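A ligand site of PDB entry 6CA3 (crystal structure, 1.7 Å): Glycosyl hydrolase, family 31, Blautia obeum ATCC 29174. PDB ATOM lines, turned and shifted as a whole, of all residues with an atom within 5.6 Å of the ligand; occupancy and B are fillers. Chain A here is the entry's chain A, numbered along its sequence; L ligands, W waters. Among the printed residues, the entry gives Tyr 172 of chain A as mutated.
The side-chain carboxylate (OD1) of Asp 423 is in hydrogen-bond range of an oxygen (O3) of the ligand, 2.4 Å away.
An oxygen (O2) of the ligand lies within hydrogen-bond range of the side-chain carboxylate of Asp 200 (2.5 Å).
A nitrogen (N1) of the ligand lies within salt-bridge range of the side-chain carboxylate of Asp 310, 2.8 Å away.
A ring nitrogen (NE2) of His 481 lies within hydrogen-bond range of an oxygen (O5) of the ligand (2.9 Å).
An oxygen (O1) of the ligand lies within hydrogen-bond range of the indole nitrogen (NE1) of Trp 274 (3.0 Å).
An oxygen (O3) of the ligand sits at hydrogen-bond distance from the guanidinium group (NH2) of Arg 407 (3.2 Å).
O1 of the ligand sits close to SD of Met 311 (3.6 Å).
The guanidinium group (NH2) of Arg 407 is in salt-bridge range of the side-chain carboxylate (OD2) of Asp 423.
OH of Tyr 88 is in hydrogen-bond range of N of Asp 423.
NE of Arg 407 lies within salt-bridge range of OD1 of Asp 310 (3.4 Å).
The guanidinium group (NH1) of Arg 407 sits at hydrogen-bond distance from the side-chain sulfur (SD) of Met 311 (3.6 Å).
NH1 of Arg 407 lies within salt-bridge range of OD2 of Asp 76 (3.4 Å).
N of Tyr 172 sits at hydrogen-bond distance from O of Ala 482.
CD2 of Tyr 172 touches C2 of the ligand, at 3.6 Å.
CG2 of Ile 201 touches O2 of the ligand, at 3.6 Å.
CD1 of Ile 237 touches O2 of the ligand, 3.9 Å away.
Trp 308 touches the ligand (CZ3 to O4, 3.6 Å).
Trp 420 touches the ligand (CZ2 to O3, 3.5 Å).
CE1 of Phe 456 touches O5 of the ligand, 3.5 Å away.
Hydrophobic or aromatic side chains within 4 Å of the ligand: Tyr 172, Ile 201, Ile 237, Trp 274, Trp 308, Met 311, Trp 420, Phe 456 and His 481.
Within 4 Å of the ligand: Tyr 172, Asp 200, Ile 201, Ile 237, Trp 274, Trp 308, Asp 310, Met 311, Arg 407, Trp 420, Asp 423, Phe 456 and His 481.
Water W3 lies within hydrogen-bond range of the side-chain carboxylate (OD2) of Asp 239, the side-chain carboxylate (OD2) of Asp 310 and an oxygen (O2) of the ligand.
Water W2 lies within hydrogen-bond range of the side-chain carboxylate (OD2) of Asp 76 (2.8 Å), the guanidinium group (NH2) of Arg 407 (2.9 Å), an oxygen (O1) of the ligand (3.1 Å) and the side-chain sulfur (SD) of Met 311 (3.5 Å).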
ATOM      1  N   ASP A  76      26.218 -26.978  20.831  1.00  0.00           N
ATOM      2  CA  ASP A  76      26.450 -25.752  21.580  1.00  0.00           C
ATOM      3  C   ASP A  76      27.316 -24.834  20.748  1.00  0.00           C
ATOM      4  O   ASP A  76      28.538 -24.969  20.719  1.00  0.00           O
ATOM      5  CB  ASP A  76      27.113 -26.069  22.926  1.00  0.00           C
ATOM      6  CG  ASP A  76      27.436 -24.824  23.732  1.00  0.00           C
ATOM      7  OD1 ASP A  76      27.048 -23.708  23.317  1.00  0.00           O
ATOM      8  OD2 ASP A  76      28.086 -24.973  24.776  1.00  0.00           O
ATOM      9  N   TYR A  88      20.835 -25.663  18.468  1.00  0.00           N
ATOM     10  CA  TYR A  88      20.614 -26.490  19.661  1.00  0.00           C
ATOM     11  C   TYR A  88      19.509 -27.532  19.478  1.00  0.00           C
ATOM     12  O   TYR A  88      19.445 -28.511  20.228  1.00  0.00           O
ATOM     13  CB  TYR A  88      20.254 -25.617  20.872  1.00  0.00           C
ATOM     14  CG  TYR A  88      21.163 -24.420  21.058  1.00  0.00           C
ATOM     15  CD1 TYR A  88      22.354 -24.517  21.780  1.00  0.00           C
ATOM     16  CD2 TYR A  88      20.814 -23.189  20.514  1.00  0.00           C
ATOM     17  CE1 TYR A  88      23.175 -23.420  21.947  1.00  0.00           C
ATOM     18  CE2 TYR A  88      21.639 -22.084  20.676  1.00  0.00           C
ATOM     19  CZ  TYR A  88      22.806 -22.205  21.385  1.00  0.00           C
ATOM     20  OH  TYR A  88      23.605 -21.093  21.537  1.00  0.00           O
ATOM     21  N   TYR A 172      24.085 -13.686  33.400  1.00  0.00           N
ATOM     22  CA  TYR A 172      25.155 -14.552  33.843  1.00  0.00           C
ATOM     23  C   TYR A 172      26.079 -13.663  34.679  1.00  0.00           C
ATOM     24  O   TYR A 172      26.865 -12.873  34.135  1.00  0.00           O
ATOM     25  CB  TYR A 172      25.893 -15.159  32.647  1.00  0.00           C
ATOM     26  CG  TYR A 172      26.978 -16.157  33.026  1.00  0.00           C
ATOM     27  CD1 TYR A 172      27.155 -16.579  34.335  1.00  0.00           C
ATOM     28  CD2 TYR A 172      27.830 -16.683  32.051  1.00  0.00           C
ATOM     29  CE1 TYR A 172      28.143 -17.482  34.683  1.00  0.00           C
ATOM     30  CE2 TYR A 172      28.830 -17.584  32.391  1.00  0.00           C
ATOM     31  CZ  TYR A 172      28.975 -17.977  33.699  1.00  0.00           C
ATOM     32  OH  TYR A 172      29.965 -18.868  34.029  1.00  0.00           O
ATOM     33  N   ASP A 200      21.334 -17.693  37.443  1.00  0.00           N
ATOM     34  CA  ASP A 200      22.269 -18.477  36.653  1.00  0.00           C
ATOM     35  C   ASP A 200      23.205 -19.251  37.583  1.00  0.00           C
ATOM     36  O   ASP A 200      23.058 -19.194  38.807  1.00  0.00           O
ATOM     37  CB  ASP A 200      23.050 -17.557  35.702  1.00  0.00           C
ATOM     38  CG  ASP A 200      23.413 -18.223  34.392  1.00  0.00           C
ATOM     39  OD1 ASP A 200      23.785 -19.422  34.393  1.00  0.00           O
ATOM     40  OD2 ASP A 200      23.356 -17.533  33.347  1.00  0.00           O
ATOM     41  N   ILE A 201      24.178 -19.959  37.005  1.00  0.00           N
ATOM     42  CA  ILE A 201      24.924 -21.003  37.730  1.00  0.00           C
ATOM     43  C   ILE A 201      25.651 -20.586  39.016  1.00  0.00           C
ATOM     44  O   ILE A 201      26.017 -21.448  39.835  1.00  0.00           O
ATOM     45  CB  ILE A 201      25.930 -21.725  36.796  1.00  0.00           C
ATOM     46  CG1 ILE A 201      26.930 -20.730  36.210  1.00  0.00           C
ATOM     47  CG2 ILE A 201      25.183 -22.446  35.667  1.00  0.00           C
ATOM     48  CD1 ILE A 201      27.937 -21.364  35.269  1.00  0.00           C
ATOM     49  N   ILE A 237      18.686 -22.123  37.337  1.00  0.00           N
ATOM     50  CA  ILE A 237      19.150 -22.956  36.242  1.00  0.00           C
ATOM     51  C   ILE A 237      19.588 -24.322  36.773  1.00  0.00           C
ATOM     52  O   ILE A 237      20.035 -24.440  37.919  1.00  0.00           O
ATOM     53  CB  ILE A 237      20.329 -22.241  35.520  1.00  0.00           C
ATOM     54  CG1 ILE A 237      20.616 -22.850  34.141  1.00  0.00           C
ATOM     55  CG2 ILE A 237      21.571 -22.202  36.399  1.00  0.00           C
ATOM     56  CD1 ILE A 237      21.648 -22.015  33.350  1.00  0.00           C
ATOM     57  N   ASP A 239      21.967 -27.678  35.207  1.00  0.00           N
ATOM     58  CA  ASP A 239      22.823 -28.135  34.105  1.00  0.00           C
ATOM     59  C   ASP A 239      22.847 -29.655  33.977  1.00  0.00           C
ATOM     60  O   ASP A 239      22.540 -30.378  34.915  1.00  0.00           O
ATOM     61  CB  ASP A 239      24.253 -27.609  34.285  1.00  0.00           C
ATOM     62  CG  ASP A 239      24.422 -26.164  33.842  1.00  0.00           C
ATOM     63  OD1 ASP A 239      23.414 -25.525  33.500  1.00  0.00           O
ATOM     64  OD2 ASP A 239      25.568 -25.659  33.857  1.00  0.00           O
ATOM     65  N   TRP A 274      31.193 -26.671  33.686  1.00  0.00           N
ATOM     66  CA  TRP A 274      31.430 -25.628  34.709  1.00  0.00           C
ATOM     67  C   TRP A 274      32.039 -26.078  36.050  1.00  0.00           C
ATOM     68  O   TRP A 274      32.932 -25.416  36.559  1.00  0.00           O
ATOM     69  CB  TRP A 274      30.189 -24.744  34.904  1.00  0.00           C
ATOM     70  CG  TRP A 274      30.000 -23.831  33.721  1.00  0.00           C
ATOM     71  CD1 TRP A 274      29.022 -23.903  32.762  1.00  0.00           C
ATOM     72  CD2 TRP A 274      30.838 -22.746  33.353  1.00  0.00           C
ATOM     73  NE1 TRP A 274      29.211 -22.912  31.836  1.00  0.00           N
ATOM     74  CE2 TRP A 274      30.317 -22.185  32.178  1.00  0.00           C
ATOM     75  CE3 TRP A 274      31.991 -22.184  33.909  1.00  0.00           C
ATOM     76  CZ2 TRP A 274      30.906 -21.077  31.543  1.00  0.00           C
ATOM     77  CZ3 TRP A 274      32.576 -21.084  33.280  1.00  0.00           C
ATOM     78  CH2 TRP A 274      32.030 -20.543  32.116  1.00  0.00           C
ATOM     79  N   TRP A 308      15.087 -23.434  34.450  1.00  0.00           N
ATOM     80  CA  TRP A 308      15.597 -23.568  33.081  1.00  0.00           C
ATOM     81  C   TRP A 308      16.758 -24.569  33.019  1.00  0.00           C
ATOM     82  O   TRP A 308      17.581 -24.614  33.923  1.00  0.00           O
ATOM     83  CB  TRP A 308      15.943 -22.217  32.427  1.00  0.00           C
ATOM     84  CG  TRP A 308      16.798 -21.251  33.208  1.00  0.00           C
ATOM     85  CD1 TRP A 308      16.655 -20.882  34.522  1.00  0.00           C
ATOM     86  CD2 TRP A 308      17.910 -20.494  32.705  1.00  0.00           C
ATOM     87  NE1 TRP A 308      17.621 -19.961  34.866  1.00  0.00           N
ATOM     88  CE2 TRP A 308      18.412 -19.709  33.764  1.00  0.00           C
ATOM     89  CE3 TRP A 308      18.545 -20.412  31.453  1.00  0.00           C
ATOM     90  CZ2 TRP A 308      19.497 -18.847  33.620  1.00  0.00           C
ATOM     91  CZ3 TRP A 308      19.634 -19.564  31.311  1.00  0.00           C
ATOM     92  CH2 TRP A 308      20.091 -18.788  32.379  1.00  0.00           C
ATOM     93  N   ASP A 310      20.026 -26.121  31.052  1.00  0.00           N
ATOM     94  CA  ASP A 310      21.054 -25.578  30.164  1.00  0.00           C
ATOM     95  C   ASP A 310      22.114 -26.643  29.878  1.00  0.00           C
ATOM     96  O   ASP A 310      22.172 -27.659  30.570  1.00  0.00           O
ATOM     97  CB  ASP A 310      21.697 -24.353  30.836  1.00  0.00           C
ATOM     98  CG  ASP A 310      22.675 -23.617  29.940  1.00  0.00           C
ATOM     99  OD1 ASP A 310      22.503 -23.664  28.703  1.00  0.00           O
ATOM    100  OD2 ASP A 310      23.609 -22.968  30.477  1.00  0.00           O
ATOM    101  N   MET A 311      22.944 -26.397  28.852  1.00  0.00           N
ATOM    102  CA  MET A 311      24.089 -27.265  28.552  1.00  0.00           C
ATOM    103  C   MET A 311      23.687 -28.700  28.231  1.00  0.00           C
ATOM    104  O   MET A 311      24.498 -29.624  28.379  1.00  0.00           O
ATOM    105  CB  MET A 311      25.099 -27.233  29.705  1.00  0.00           C
ATOM    106  CG  MET A 311      25.591 -25.841  30.069  1.00  0.00           C
ATOM    107  SD  MET A 311      26.623 -25.136  28.770  1.00  0.00           S
ATOM    108  CE  MET A 311      28.198 -25.883  29.168  1.00  0.00           C
ATOM    109  N   PHE A 317      33.253 -29.275  27.559  1.00  0.00           N
ATOM    110  CA  PHE A 317      34.411 -28.403  27.311  1.00  0.00           C
ATOM    111  C   PHE A 317      35.574 -29.255  26.856  1.00  0.00           C
ATOM    112  O   PHE A 317      36.350 -28.865  25.979  1.00  0.00           O
ATOM    113  CB  PHE A 317      34.806 -27.608  28.552  1.00  0.00           C
ATOM    114  CG  PHE A 317      33.763 -26.638  29.036  1.00  0.00           C
ATOM    115  CD1 PHE A 317      32.669 -26.298  28.239  1.00  0.00           C
ATOM    116  CD2 PHE A 317      33.874 -26.055  30.292  1.00  0.00           C
ATOM    117  CE1 PHE A 317      31.706 -25.410  28.685  1.00  0.00           C
ATOM    118  CE2 PHE A 317      32.909 -25.158  30.749  1.00  0.00           C
ATOM    119  CZ  PHE A 317      31.833 -24.844  29.948  1.00  0.00           C
ATOM    120  N   ARG A 407      17.368 -25.635  26.637  1.00  0.00           N
ATOM    121  CA  ARG A 407      18.126 -25.147  25.487  1.00  0.00           C
ATOM    122  C   ARG A 407      18.034 -26.118  24.315  1.00  0.00           C
ATOM    123  O   ARG A 407      17.578 -25.755  23.227  1.00  0.00           O
ATOM    124  CB  ARG A 407      19.597 -24.882  25.855  1.00  0.00           C
ATOM    125  CG  ARG A 407      20.317 -24.034  24.794  1.00  0.00           C
ATOM    126  CD  ARG A 407      21.631 -23.477  25.293  1.00  0.00           C
ATOM    127  NE  ARG A 407      22.665 -24.509  25.377  1.00  0.00           N
ATOM    128  CZ  ARG A 407      23.967 -24.246  25.559  1.00  0.00           C
ATOM    129  NH1 ARG A 407      24.844 -25.227  25.619  1.00  0.00           N
ATOM    130  NH2 ARG A 407      24.374 -22.985  25.674  1.00  0.00           N
ATOM    131  N   TRP A 420      14.245 -21.740  25.049  1.00  0.00           N
ATOM    132  CA  TRP A 420      14.677 -20.402  24.667  1.00  0.00           C
ATOM    133  C   TRP A 420      15.684 -20.550  23.531  1.00  0.00           C
ATOM    134  O   TRP A 420      16.286 -21.612  23.367  1.00  0.00           O
ATOM    135  CB  TRP A 420      15.216 -19.590  25.867  1.00  0.00           C
ATOM    136  CG  TRP A 420      16.683 -19.700  26.167  1.00  0.00           C
ATOM    137  CD1 TRP A 420      17.658 -18.799  25.808  1.00  0.00           C
ATOM    138  CD2 TRP A 420      17.341 -20.728  26.909  1.00  0.00           C
ATOM    139  NE1 TRP A 420      18.881 -19.219  26.281  1.00  0.00           N
ATOM    140  CE2 TRP A 420      18.707 -20.402  26.962  1.00  0.00           C
ATOM    141  CE3 TRP A 420      16.893 -21.894  27.543  1.00  0.00           C
ATOM    142  CZ2 TRP A 420      19.645 -21.206  27.624  1.00  0.00           C
ATOM    143  CZ3 TRP A 420      17.819 -22.695  28.200  1.00  0.00           C
ATOM    144  CH2 TRP A 420      19.184 -22.344  28.233  1.00  0.00           C
ATOM    145  N   GLY A 422      18.593 -19.829  22.902  1.00  0.00           N
ATOM    146  CA  GLY A 422      20.014 -19.995  23.165  1.00  0.00           C
ATOM    147  C   GLY A 422      20.827 -18.720  23.126  1.00  0.00           C
ATOM    148  O   GLY A 422      20.328 -17.613  23.356  1.00  0.00           O
ATOM    149  N   ASP A 423      22.110 -18.881  22.801  1.00  0.00           N
ATOM    150  CA  ASP A 423      23.062 -17.789  22.869  1.00  0.00           C
ATOM    151  C   ASP A 423      23.051 -16.971  21.585  1.00  0.00           C
ATOM    152  O   ASP A 423      23.864 -17.181  20.691  1.00  0.00           O
ATOM    153  CB  ASP A 423      24.472 -18.326  23.142  1.00  0.00           C
ATOM    154  CG  ASP A 423      24.592 -18.982  24.510  1.00  0.00           C
ATOM    155  OD1 ASP A 423      23.672 -18.804  25.336  1.00  0.00           O
ATOM    156  OD2 ASP A 423      25.591 -19.685  24.755  1.00  0.00           O
ATOM    157  N   ASP A 452      16.843 -14.318  23.958  1.00  0.00           N
ATOM    158  CA  ASP A 452      17.470 -13.423  24.944  1.00  0.00           C
ATOM    159  C   ASP A 452      17.339 -11.997  24.461  1.00  0.00           C
ATOM    160  O   ASP A 452      18.051 -11.565  23.538  1.00  0.00           O
ATOM    161  CB  ASP A 452      18.950 -13.778  25.132  1.00  0.00           C
ATOM    162  CG  ASP A 452      19.148 -15.049  25.943  1.00  0.00           C
ATOM    163  OD1 ASP A 452      18.150 -15.574  26.502  1.00  0.00           O
ATOM    164  OD2 ASP A 452      20.307 -15.527  26.040  1.00  0.00           O
ATOM    165  N   PHE A 456      22.148 -11.938  23.968  1.00  0.00           N
ATOM    166  CA  PHE A 456      23.003 -12.555  24.986  1.00  0.00           C
ATOM    167  C   PHE A 456      24.452 -12.076  24.904  1.00  0.00           C
ATOM    168  O   PHE A 456      24.967 -11.421  25.824  1.00  0.00           O
ATOM    169  CB  PHE A 456      22.955 -14.074  24.843  1.00  0.00           C
ATOM    170  CG  PHE A 456      23.811 -14.814  25.840  1.00  0.00           C
ATOM    171  CD1 PHE A 456      23.484 -14.812  27.193  1.00  0.00           C
ATOM    172  CD2 PHE A 456      24.930 -15.522  25.427  1.00  0.00           C
ATOM    173  CE1 PHE A 456      24.250 -15.507  28.111  1.00  0.00           C
ATOM    174  CE2 PHE A 456      25.726 -16.216  26.349  1.00  0.00           C
ATOM    175  CZ  PHE A 456      25.383 -16.197  27.695  1.00  0.00           C
ATOM    176  N   ARG A 479      12.182 -12.432  28.102  1.00  0.00           N
ATOM    177  CA  ARG A 479      13.292 -12.409  29.051  1.00  0.00           C
ATOM    178  C   ARG A 479      14.481 -11.653  28.509  1.00  0.00           C
ATOM    179  O   ARG A 479      14.990 -11.968  27.430  1.00  0.00           O
ATOM    180  CB  ARG A 479      13.715 -13.848  29.390  1.00  0.00           C
ATOM    181  CG  ARG A 479      14.906 -13.928  30.345  1.00  0.00           C
ATOM    182  CD  ARG A 479      15.327 -15.365  30.610  1.00  0.00           C
ATOM    183  NE  ARG A 479      16.131 -15.940  29.547  1.00  0.00           N
ATOM    184  CZ  ARG A 479      16.978 -16.953  29.728  1.00  0.00           C
ATOM    185  NH1 ARG A 479      17.107 -17.500  30.937  1.00  0.00           N
ATOM    186  NH2 ARG A 479      17.701 -17.422  28.720  1.00  0.00           N
ATOM    187  N   HIS A 481      18.228 -11.256  28.908  1.00  0.00           N
ATOM    188  CA  HIS A 481      19.348 -12.034  29.437  1.00  0.00           C
ATOM    189  C   HIS A 481      20.658 -11.617  28.767  1.00  0.00           C
ATOM    190  O   HIS A 481      20.664 -11.220  27.594  1.00  0.00           O
ATOM    191  CB  HIS A 481      19.095 -13.532  29.212  1.00  0.00           C
ATOM    192  CG  HIS A 481      20.139 -14.423  29.808  1.00  0.00           C
ATOM    193  ND1 HIS A 481      20.589 -14.293  31.104  1.00  0.00           N
ATOM    194  CD2 HIS A 481      20.796 -15.493  29.294  1.00  0.00           C
ATOM    195  CE1 HIS A 481      21.492 -15.220  31.355  1.00  0.00           C
ATOM    196  NE2 HIS A 481      21.639 -15.956  30.278  1.00  0.00           N
ATOM    197  N   ALA A 482      21.760 -11.688  29.516  1.00  0.00           N
ATOM    198  CA  ALA A 482      23.055 -11.199  29.032  1.00  0.00           C
ATOM    199  C   ALA A 482      24.214 -12.061  29.526  1.00  0.00           C
ATOM    200  O   ALA A 482      24.176 -12.612  30.625  1.00  0.00           O
ATOM    201  CB  ALA A 482      23.262  -9.765  29.474  1.00  0.00           C
HETATM  202  O1  LIG L   1      28.783 -22.283  28.951  1.00  0.00           O
HETATM  203  O2  LIG L   1      25.160 -20.522  32.622  1.00  0.00           O
HETATM  204  O3  LIG L   1      22.952 -20.430  27.008  1.00  0.00           O
HETATM  205  O4  LIG L   1      22.014 -18.618  28.850  1.00  0.00           O
HETATM  206  O5  LIG L   1      23.898 -17.756  30.831  1.00  0.00           O
HETATM  207  C1  LIG L   1      27.821 -21.335  29.312  1.00  0.00           C
HETATM  208  C2  LIG L   1      25.831 -19.674  31.809  1.00  0.00           C
HETATM  209  C3  LIG L   1      26.578 -21.764  29.941  1.00  0.00           C
HETATM  210  C4  LIG L   1      24.797 -21.020  28.400  1.00  0.00           C
HETATM  211  C5  LIG L   1      23.404 -20.419  28.344  1.00  0.00           C
HETATM  212  C6  LIG L   1      23.343 -19.065  28.909  1.00  0.00           C
HETATM  213  C7  LIG L   1      23.886 -19.055  30.310  1.00  0.00           C
HETATM  214  C8  LIG L   1      25.309 -19.609  30.379  1.00  0.00           C
HETATM  215  N1  LIG L   1      25.419 -20.923  29.756  1.00  0.00           N
HETATM  216  O   HOH W   1      21.443 -17.773  26.453  1.00  0.00           O
HETATM  217  O   HOH W   2      27.191 -22.755  26.322  1.00  0.00           O
HETATM  218  O   HOH W   3      25.233 -23.511  32.532  1.00  0.00           O
